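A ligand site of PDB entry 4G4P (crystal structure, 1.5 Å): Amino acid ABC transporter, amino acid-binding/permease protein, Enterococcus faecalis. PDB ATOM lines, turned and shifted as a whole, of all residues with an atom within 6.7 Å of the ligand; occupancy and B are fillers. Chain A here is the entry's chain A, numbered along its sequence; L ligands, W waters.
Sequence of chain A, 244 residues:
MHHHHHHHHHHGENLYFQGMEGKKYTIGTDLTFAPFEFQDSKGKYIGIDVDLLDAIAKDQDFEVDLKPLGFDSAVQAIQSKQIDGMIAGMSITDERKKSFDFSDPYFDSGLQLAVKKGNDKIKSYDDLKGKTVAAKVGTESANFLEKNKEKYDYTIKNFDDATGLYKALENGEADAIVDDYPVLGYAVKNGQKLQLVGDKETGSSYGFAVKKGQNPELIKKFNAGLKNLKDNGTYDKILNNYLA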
ATOM      1  N   ASP A  30       1.669  -0.528  27.245  1.00  0.00           N
ATOM      2  CA  ASP A  30       2.420  -0.107  26.070  1.00  0.00           C
ATOM      3  C   ASP A  30       3.208   1.167  26.393  1.00  0.00           C
ATOM      4  O   ASP A  30       2.929   1.856  27.376  1.00  0.00           O
ATOM      5  CB  ASP A  30       1.430   0.109  24.914  1.00  0.00           C
ATOM      6  CG  ASP A  30       2.073   0.084  23.524  1.00  0.00           C
ATOM      7  OD1 ASP A  30       3.320   0.025  23.374  1.00  0.00           O
ATOM      8  OD2 ASP A  30       1.270   0.147  22.562  1.00  0.00           O
ATOM      9  N   THR A  32       3.664   3.989  24.327  1.00  0.00           N
ATOM     10  CA  THR A  32       2.750   5.078  24.012  1.00  0.00           C
ATOM     11  C   THR A  32       1.671   4.536  23.073  1.00  0.00           C
ATOM     12  O   THR A  32       1.950   3.847  22.091  1.00  0.00           O
ATOM     13  CB  THR A  32       3.448   6.321  23.411  1.00  0.00           C
ATOM     14  OG1 THR A  32       2.458   7.364  23.250  1.00  0.00           O
ATOM     15  CG2 THR A  32       4.134   6.015  22.097  1.00  0.00           C
ATOM     16  N   PHE A  33       0.438   4.831  23.425  1.00  0.00           N
ATOM     17  CA  PHE A  33      -0.730   4.317  22.710  1.00  0.00           C
ATOM     18  C   PHE A  33      -1.881   5.248  23.066  1.00  0.00           C
ATOM     19  O   PHE A  33      -2.862   4.857  23.683  1.00  0.00           O
ATOM     20  CB  PHE A  33      -1.008   2.879  23.132  1.00  0.00           C
ATOM     21  CG  PHE A  33      -1.905   2.121  22.187  1.00  0.00           C
ATOM     22  CD1 PHE A  33      -1.560   1.982  20.851  1.00  0.00           C
ATOM     23  CD2 PHE A  33      -3.067   1.490  22.627  1.00  0.00           C
ATOM     24  CE1 PHE A  33      -2.368   1.280  19.971  1.00  0.00           C
ATOM     25  CE2 PHE A  33      -3.864   0.787  21.738  1.00  0.00           C
ATOM     26  CZ  PHE A  33      -3.495   0.668  20.422  1.00  0.00           C
ATOM     27  N   GLU A  37      -2.747   4.998  26.836  1.00  0.00           N
ATOM     28  CA  GLU A  37      -1.638   5.287  27.731  1.00  0.00           C
ATOM     29  C   GLU A  37      -0.603   6.112  26.993  1.00  0.00           C
ATOM     30  O   GLU A  37      -0.320   5.878  25.816  1.00  0.00           O
ATOM     31  CB  GLU A  37      -0.979   4.031  28.301  1.00  0.00           C
ATOM     32  CG  GLU A  37      -0.628   2.950  27.294  1.00  0.00           C
ATOM     33  CD  GLU A  37      -1.732   1.964  27.086  1.00  0.00           C
ATOM     34  OE1 GLU A  37      -2.671   1.946  27.884  1.00  0.00           O
ATOM     35  OE2 GLU A  37      -1.658   1.191  26.099  1.00  0.00           O
ATOM     36  N   GLY A  70       5.860  -1.913  26.326  1.00  0.00           N
ATOM     37  CA  GLY A  70       5.570  -2.090  24.911  1.00  0.00           C
ATOM     38  C   GLY A  70       4.604  -3.236  24.782  1.00  0.00           C
ATOM     39  O   GLY A  70       4.536  -4.109  25.647  1.00  0.00           O
ATOM     40  N   PHE A  71       3.831  -3.243  23.715  1.00  0.00           N
ATOM     41  CA  PHE A  71       2.739  -4.188  23.635  1.00  0.00           C
ATOM     42  C   PHE A  71       3.194  -5.644  23.583  1.00  0.00           C
ATOM     43  O   PHE A  71       2.817  -6.430  24.434  1.00  0.00           O
ATOM     44  CB  PHE A  71       1.781  -3.884  22.487  1.00  0.00           C
ATOM     45  CG  PHE A  71       0.615  -4.832  22.464  1.00  0.00           C
ATOM     46  CD1 PHE A  71      -0.423  -4.689  23.380  1.00  0.00           C
ATOM     47  CD2 PHE A  71       0.614  -5.931  21.628  1.00  0.00           C
ATOM     48  CE1 PHE A  71      -1.464  -5.609  23.403  1.00  0.00           C
ATOM     49  CE2 PHE A  71      -0.421  -6.840  21.658  1.00  0.00           C
ATOM     50  CZ  PHE A  71      -1.460  -6.679  22.546  1.00  0.00           C
ATOM     51  N   ALA A  88      -3.405  -2.457  27.940  1.00  0.00           N
ATOM     52  CA  ALA A  88      -2.640  -1.860  26.843  1.00  0.00           C
ATOM     53  C   ALA A  88      -3.466  -1.797  25.585  1.00  0.00           C
ATOM     54  O   ALA A  88      -3.016  -2.161  24.499  1.00  0.00           O
ATOM     55  CB  ALA A  88      -1.344  -2.667  26.570  1.00  0.00           C
ATOM     56  N   GLY A  89      -4.713  -1.336  25.724  1.00  0.00           N
ATOM     57  CA  GLY A  89      -5.629  -1.340  24.593  1.00  0.00           C
ATOM     58  C   GLY A  89      -5.642  -2.693  23.910  1.00  0.00           C
ATOM     59  O   GLY A  89      -5.556  -2.778  22.681  1.00  0.00           O
ATOM     60  N   MET A  90      -5.758  -3.739  24.724  1.00  0.00           N
ATOM     61  CA  MET A  90      -5.574  -5.111  24.240  1.00  0.00           C
ATOM     62  C   MET A  90      -6.868  -5.756  23.782  1.00  0.00           C
ATOM     63  O   MET A  90      -7.813  -5.936  24.560  1.00  0.00           O
ATOM     64  CB  MET A  90      -4.959  -5.975  25.329  1.00  0.00           C
ATOM     65  CG  MET A  90      -4.610  -7.358  24.857  1.00  0.00           C
ATOM     66  SD  MET A  90      -3.717  -8.223  26.145  1.00  0.00           S
ATOM     67  CE  MET A  90      -3.271  -9.735  25.294  1.00  0.00           C
ATOM     68  N   SER A  91      -6.889  -6.158  22.515  1.00  0.00           N
ATOM     69  CA  SER A  91      -8.058  -6.799  21.937  1.00  0.00           C
ATOM     70  C   SER A  91      -8.290  -8.200  22.477  1.00  0.00           C
ATOM     71  O   SER A  91      -7.379  -9.030  22.498  1.00  0.00           O
ATOM     72  CB  SER A  91      -7.892  -6.886  20.423  1.00  0.00           C
ATOM     73  OG  SER A  91      -7.775  -5.591  19.862  1.00  0.00           O
ATOM     74  N   ILE A  92      -9.528  -8.441  22.876  1.00  0.00           N
ATOM     75  CA  ILE A  92     -10.003  -9.776  23.230  1.00  0.00           C
ATOM     76  C   ILE A  92     -10.226 -10.548  21.946  1.00  0.00           C
ATOM     77  O   ILE A  92     -11.008 -10.123  21.091  1.00  0.00           O
ATOM     78  CB  ILE A  92     -11.312  -9.658  24.008  1.00  0.00           C
ATOM     79  CG1 ILE A  92     -11.104  -8.838  25.289  1.00  0.00           C
ATOM     80  CG2 ILE A  92     -11.847 -11.031  24.345  1.00  0.00           C
ATOM     81  CD1 ILE A  92     -12.419  -8.425  25.966  1.00  0.00           C
ATOM     82  N   THR A  93      -9.522 -11.654  21.784  1.00  0.00           N
ATOM     83  CA  THR A  93      -9.690 -12.493  20.599  1.00  0.00           C
ATOM     84  C   THR A  93      -9.764 -13.952  21.013  1.00  0.00           C
ATOM     85  O   THR A  93      -9.246 -14.342  22.067  1.00  0.00           O
ATOM     86  CB  THR A  93      -8.546 -12.338  19.579  1.00  0.00           C
ATOM     87  OG1 THR A  93      -7.365 -12.984  20.085  1.00  0.00           O
ATOM     88  CG2 THR A  93      -8.263 -10.874  19.243  1.00  0.00           C
ATOM     89  N   ARG A  96      -6.314 -15.475  21.458  1.00  0.00           N
ATOM     90  CA  ARG A  96      -5.654 -15.061  22.682  1.00  0.00           C
ATOM     91  C   ARG A  96      -6.266 -15.712  23.926  1.00  0.00           C
ATOM     92  O   ARG A  96      -5.557 -15.915  24.912  1.00  0.00           O
ATOM     93  CB  ARG A  96      -5.636 -13.542  22.831  1.00  0.00           C
ATOM     94  CG  ARG A  96      -4.700 -12.883  21.861  1.00  0.00           C
ATOM     95  CD  ARG A  96      -4.866 -11.382  21.857  1.00  0.00           C
ATOM     96  NE  ARG A  96      -3.842 -10.739  21.034  1.00  0.00           N
ATOM     97  CZ  ARG A  96      -3.766  -9.444  20.826  1.00  0.00           C
ATOM     98  NH1 ARG A  96      -4.690  -8.640  21.331  1.00  0.00           N
ATOM     99  NH2 ARG A  96      -2.783  -8.944  20.100  1.00  0.00           N
ATOM    100  N   SER A 109     -13.287  -1.203  19.614  1.00  0.00           N
ATOM    101  CA  SER A 109     -12.234  -0.726  18.760  1.00  0.00           C
ATOM    102  C   SER A 109     -12.207  -1.482  17.430  1.00  0.00           C
ATOM    103  O   SER A 109     -13.187  -2.129  17.039  1.00  0.00           O
ATOM    104  CB  SER A 109     -10.886  -0.842  19.500  1.00  0.00           C
ATOM    105  OG  SER A 109      -9.888  -0.107  18.833  1.00  0.00           O
ATOM    106  N   GLY A 110     -11.102  -1.337  16.719  1.00  0.00           N
ATOM    107  CA  GLY A 110     -10.912  -1.946  15.421  1.00  0.00           C
ATOM    108  C   GLY A 110      -9.628  -1.414  14.837  1.00  0.00           C
ATOM    109  O   GLY A 110      -8.857  -0.755  15.541  1.00  0.00           O
ATOM    110  N   LEU A 111      -9.418  -1.677  13.553  1.00  0.00           N
ATOM    111  CA  LEU A 111      -8.197  -1.279  12.855  1.00  0.00           C
ATOM    112  C   LEU A 111      -8.476  -0.209  11.799  1.00  0.00           C
ATOM    113  O   LEU A 111      -9.579  -0.092  11.297  1.00  0.00           O
ATOM    114  CB  LEU A 111      -7.576  -2.499  12.178  1.00  0.00           C
ATOM    115  CG  LEU A 111      -7.320  -3.695  13.089  1.00  0.00           C
ATOM    116  CD1 LEU A 111      -6.753  -4.875  12.284  1.00  0.00           C
ATOM    117  CD2 LEU A 111      -6.388  -3.315  14.234  1.00  0.00           C
ATOM    118  N   LYS A 136       2.839  -2.541  14.263  1.00  0.00           N
ATOM    119  CA  LYS A 136       3.584  -2.912  15.445  1.00  0.00           C
ATOM    120  C   LYS A 136       3.583  -4.414  15.629  1.00  0.00           C
ATOM    121  O   LYS A 136       2.565  -5.086  15.455  1.00  0.00           O
ATOM    122  CB  LYS A 136       2.979  -2.235  16.681  1.00  0.00           C
ATOM    123  CG  LYS A 136       3.261  -0.754  16.751  1.00  0.00           C
ATOM    124  CD  LYS A 136       2.188  -0.028  17.582  1.00  0.00           C
ATOM    125  CE  LYS A 136       2.223  -0.390  19.028  1.00  0.00           C
ATOM    126  NZ  LYS A 136       1.179   0.317  19.805  1.00  0.00           N
ATOM    127  N   VAL A 137       4.749  -4.949  15.979  1.00  0.00           N
ATOM    128  CA  VAL A 137       4.917  -6.372  16.263  1.00  0.00           C
ATOM    129  C   VAL A 137       3.858  -6.909  17.216  1.00  0.00           C
ATOM    130  O   VAL A 137       3.525  -6.284  18.230  1.00  0.00           O
ATOM    131  CB  VAL A 137       6.293  -6.640  16.909  1.00  0.00           C
ATOM    132  CG1 VAL A 137       6.416  -8.074  17.397  1.00  0.00           C
ATOM    133  CG2 VAL A 137       7.385  -6.380  15.934  1.00  0.00           C
ATOM    134  N   GLY A 138       3.326  -8.088  16.892  1.00  0.00           N
ATOM    135  CA  GLY A 138       2.525  -8.810  17.838  1.00  0.00           C
ATOM    136  C   GLY A 138       1.122  -8.302  18.045  1.00  0.00           C
ATOM    137  O   GLY A 138       0.425  -8.762  18.928  1.00  0.00           O
ATOM    138  N   THR A 139       0.691  -7.364  17.197  1.00  0.00           N
ATOM    139  CA  THR A 139      -0.610  -6.734  17.371  1.00  0.00           C
ATOM    140  C   THR A 139      -1.623  -7.278  16.390  1.00  0.00           C
ATOM    141  O   THR A 139      -1.279  -7.958  15.423  1.00  0.00           O
ATOM    142  CB  THR A 139      -0.533  -5.211  17.130  1.00  0.00           C
ATOM    143  OG1 THR A 139      -0.118  -4.974  15.775  1.00  0.00           O
ATOM    144  CG2 THR A 139       0.452  -4.552  18.090  1.00  0.00           C
ATOM    145  N   GLU A 140      -2.887  -6.940  16.633  1.00  0.00           N
ATOM    146  CA  GLU A 140      -3.938  -7.241  15.674  1.00  0.00           C
ATOM    147  C   GLU A 140      -3.665  -6.612  14.307  1.00  0.00           C
ATOM    148  O   GLU A 140      -4.010  -7.206  13.264  1.00  0.00           O
ATOM    149  CB  GLU A 140      -5.282  -6.792  16.235  1.00  0.00           C
ATOM    150  CG  GLU A 140      -5.692  -7.705  17.397  1.00  0.00           C
ATOM    151  CD  GLU A 140      -5.814  -9.179  16.954  1.00  0.00           C
ATOM    152  OE1 GLU A 140      -6.695  -9.441  16.115  1.00  0.00           O
ATOM    153  OE2 GLU A 140      -5.031 -10.087  17.426  1.00  0.00           O
ATOM    154  N   SER A 141      -3.062  -5.426  14.283  1.00  0.00           N
ATOM    155  CA  SER A 141      -2.688  -4.825  13.011  1.00  0.00           C
ATOM    156  C   SER A 141      -1.683  -5.709  12.267  1.00  0.00           C
ATOM    157  O   SER A 141      -1.785  -5.886  11.060  1.00  0.00           O
ATOM    158  CB  SER A 141      -2.091  -3.424  13.210  1.00  0.00           C
ATOM    159  OG  SER A 141      -3.080  -2.505  13.670  1.00  0.00           O
ATOM    160  N   ASP A 179      -3.001   0.669  12.383  1.00  0.00           N
ATOM    161  CA  ASP A 179      -2.990   0.757  13.851  1.00  0.00           C
ATOM    162  C   ASP A 179      -4.434   0.804  14.299  1.00  0.00           C
ATOM    163  O   ASP A 179      -5.356   0.832  13.469  1.00  0.00           O
ATOM    164  CB  ASP A 179      -2.218   2.018  14.311  1.00  0.00           C
ATOM    165  CG  ASP A 179      -1.714   1.926  15.771  1.00  0.00           C
ATOM    166  OD1 ASP A 179      -2.062   0.960  16.483  1.00  0.00           O
ATOM    167  OD2 ASP A 179      -0.986   2.861  16.207  1.00  0.00           O
ATOM    168  N   ASP A 180      -4.668   0.836  15.597  1.00  0.00           N
ATOM    169  CA  ASP A 180      -6.052   0.834  16.051  1.00  0.00           C
ATOM    170  C   ASP A 180      -6.800   2.118  15.691  1.00  0.00           C
ATOM    171  O   ASP A 180      -6.254   3.228  15.733  1.00  0.00           O
ATOM    172  CB  ASP A 180      -6.115   0.622  17.570  1.00  0.00           C
ATOM    173  CG  ASP A 180      -5.950  -0.839  17.975  1.00  0.00           C
ATOM    174  OD1 ASP A 180      -5.550  -1.669  17.130  1.00  0.00           O
ATOM    175  OD2 ASP A 180      -6.163  -1.138  19.171  1.00  0.00           O
ATOM    176  N   SER A 204     -13.038  -5.229  17.388  1.00  0.00           N
ATOM    177  CA  SER A 204     -12.720  -5.965  18.605  1.00  0.00           C
ATOM    178  C   SER A 204     -13.014  -5.071  19.790  1.00  0.00           C
ATOM    179  O   SER A 204     -13.310  -3.903  19.621  1.00  0.00           O
ATOM    180  CB  SER A 204     -11.276  -6.428  18.652  1.00  0.00           C
ATOM    181  OG  SER A 204     -10.384  -5.345  18.700  1.00  0.00           O
ATOM    182  N   TYR A 206     -11.588  -4.097  23.877  1.00  0.00           N
ATOM    183  CA  TYR A 206     -10.404  -4.165  24.736  1.00  0.00           C
ATOM    184  C   TYR A 206     -10.759  -4.794  26.075  1.00  0.00           C
ATOM    185  O   TYR A 206     -11.857  -4.574  26.609  1.00  0.00           O
ATOM    186  CB  TYR A 206      -9.833  -2.791  25.000  1.00  0.00           C
ATOM    187  CG  TYR A 206      -9.298  -2.010  23.813  1.00  0.00           C
ATOM    188  CD1 TYR A 206      -8.953  -2.619  22.620  1.00  0.00           C
ATOM    189  CD2 TYR A 206      -9.113  -0.640  23.924  1.00  0.00           C
ATOM    190  CE1 TYR A 206      -8.441  -1.880  21.576  1.00  0.00           C
ATOM    191  CE2 TYR A 206      -8.606   0.111  22.895  1.00  0.00           C
ATOM    192  CZ  TYR A 206      -8.265  -0.509  21.710  1.00  0.00           C
ATOM    193  OH  TYR A 206      -7.778   0.279  20.684  1.00  0.00           O
HETATM  194  N1  LIG L   1      -5.573  -3.637  20.106  1.00  0.00           N
HETATM  195  C1  LIG L   1      -4.345  -4.143  19.419  1.00  0.00           C
HETATM  196  C2  LIG L   1      -3.960  -5.485  19.963  1.00  0.00           C
HETATM  197  O1  LIG L   1      -4.511  -5.898  20.990  1.00  0.00           O
HETATM  198  C3  LIG L   1      -3.179  -3.175  19.570  1.00  0.00           C
HETATM  199  C4  LIG L   1      -2.636  -2.985  20.982  1.00  0.00           C
HETATM  200  C5  LIG L   1      -1.472  -2.008  21.034  1.00  0.00           C
HETATM  201  O2  LIG L   1      -0.800  -1.733  20.024  1.00  0.00           O
HETATM  202  N2  LIG L   1      -1.210  -1.471  22.225  1.00  0.00           N
HETATM  203  O3  LIG L   1      -3.119  -6.170  19.350  1.00  0.00           O
HETATM  204  O   HOH W   1      -1.214  -1.492  17.259  1.00  0.00           O
HETATM  205  O   HOH W   2      -7.356  -3.929  17.557  1.00  0.00           O
HETATM  206  O   HOH W   3      -3.306  -3.073  16.329  1.00  0.00           O
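The backbone carbonyl oxygen of Gly 89 lies within hydrogen-bond range of a nitrogen (N1) of the ligand (2.7 Å). OD2 of Asp 180 is in salt-bridge range of N1 of the ligand (2.7 Å). An oxygen (O1) of the ligand is in salt-bridge range of the guanidinium group (NH1) of Arg 96, 2.8 Å away. N of Glu 140 is in hydrogen-bond range of O3 of the ligand (2.8 Å). An oxygen (O1) of the ligand lies within hydrogen-bond range of the backbone NH of Ser 91 (2.8 Å). OG of Ser 91 sits at hydrogen-bond distance from N1 of the ligand, at 3.0 Å. The side-chain amino group (NZ) of Lys 136 lies within hydrogen-bond range of an oxygen (O2) of the ligand (2.9 Å). N2 of the ligand sits at hydrogen-bond distance from OD2 of Asp 30. O of Ala 88 sits at hydrogen-bond distance from N2 of the ligand.
OD2 of Asp 180 lies within hydrogen-bond range of OH of Tyr 206, at 2.6 Å. The guanidinium group (NH2) of Arg 96 is in hydrogen-bond range of the backbone carbonyl oxygen (O) of Gly 138. N of Arg 96 lies within hydrogen-bond range of OG1 of Thr 93 (3.0 Å). The side-chain hydroxyl of Ser 204 lies within hydrogen-bond range of the side-chain hydroxyl of Ser 91 (2.9 Å). NZ of Lys 136 lies within salt-bridge range of OD2 of Asp 30 (2.8 Å). The backbone carbonyl oxygen of Lys 136 is in hydrogen-bond range of the side-chain hydroxyl of Thr 139, at 2.7 Å. The side-chain carboxylate of Asp 30 sits at hydrogen-bond distance from the backbone NH of Phe 71, at 3.3 Å. OG1 of Thr 139 lies close to N of Ser 141 (3.3 Å).
Merely in contact with the ligand: Phe 33 (3.4 Å), Phe 71 (3.5 Å), Met 90 (3.5 Å), Thr 139 (3.2 Å) and Tyr 206 (3.7 Å). Hydrophobic or aromatic side chains within 4 Å of the ligand: Phe 33, Phe 71 and Tyr 206. 13 residues have an atom within 4 Å of the ligand: Asp 30, Phe 33, Phe 71, Ala 88, Gly 89, Met 90, Ser 91, Arg 96, Lys 136, Thr 139, Glu 140, Asp 180 and Tyr 206. Along chain A the residues within 4 Å of the ligand span positions 30 to 206. The nearest printed residue that does not touch the ligand is Gly 138 (4.4 Å).
Water W1 lies within hydrogen-bond range of the side-chain carboxylate of Asp 179 and an oxygen (O2) of the ligand. Water W2 lies within hydrogen-bond range of the side-chain hydroxyl (OG) of Ser 91 (2.9 Å), the side-chain carboxylate (OD1) of Asp 180 (2.9 Å) and a nitrogen (N1) of the ligand (3.1 Å). Water W3 lies within hydrogen-bond range of the side-chain hydroxyl (OG) of Ser 141 (2.7 Å) and the side-chain carboxylate (OD1) of Asp 180 (2.8 Å).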
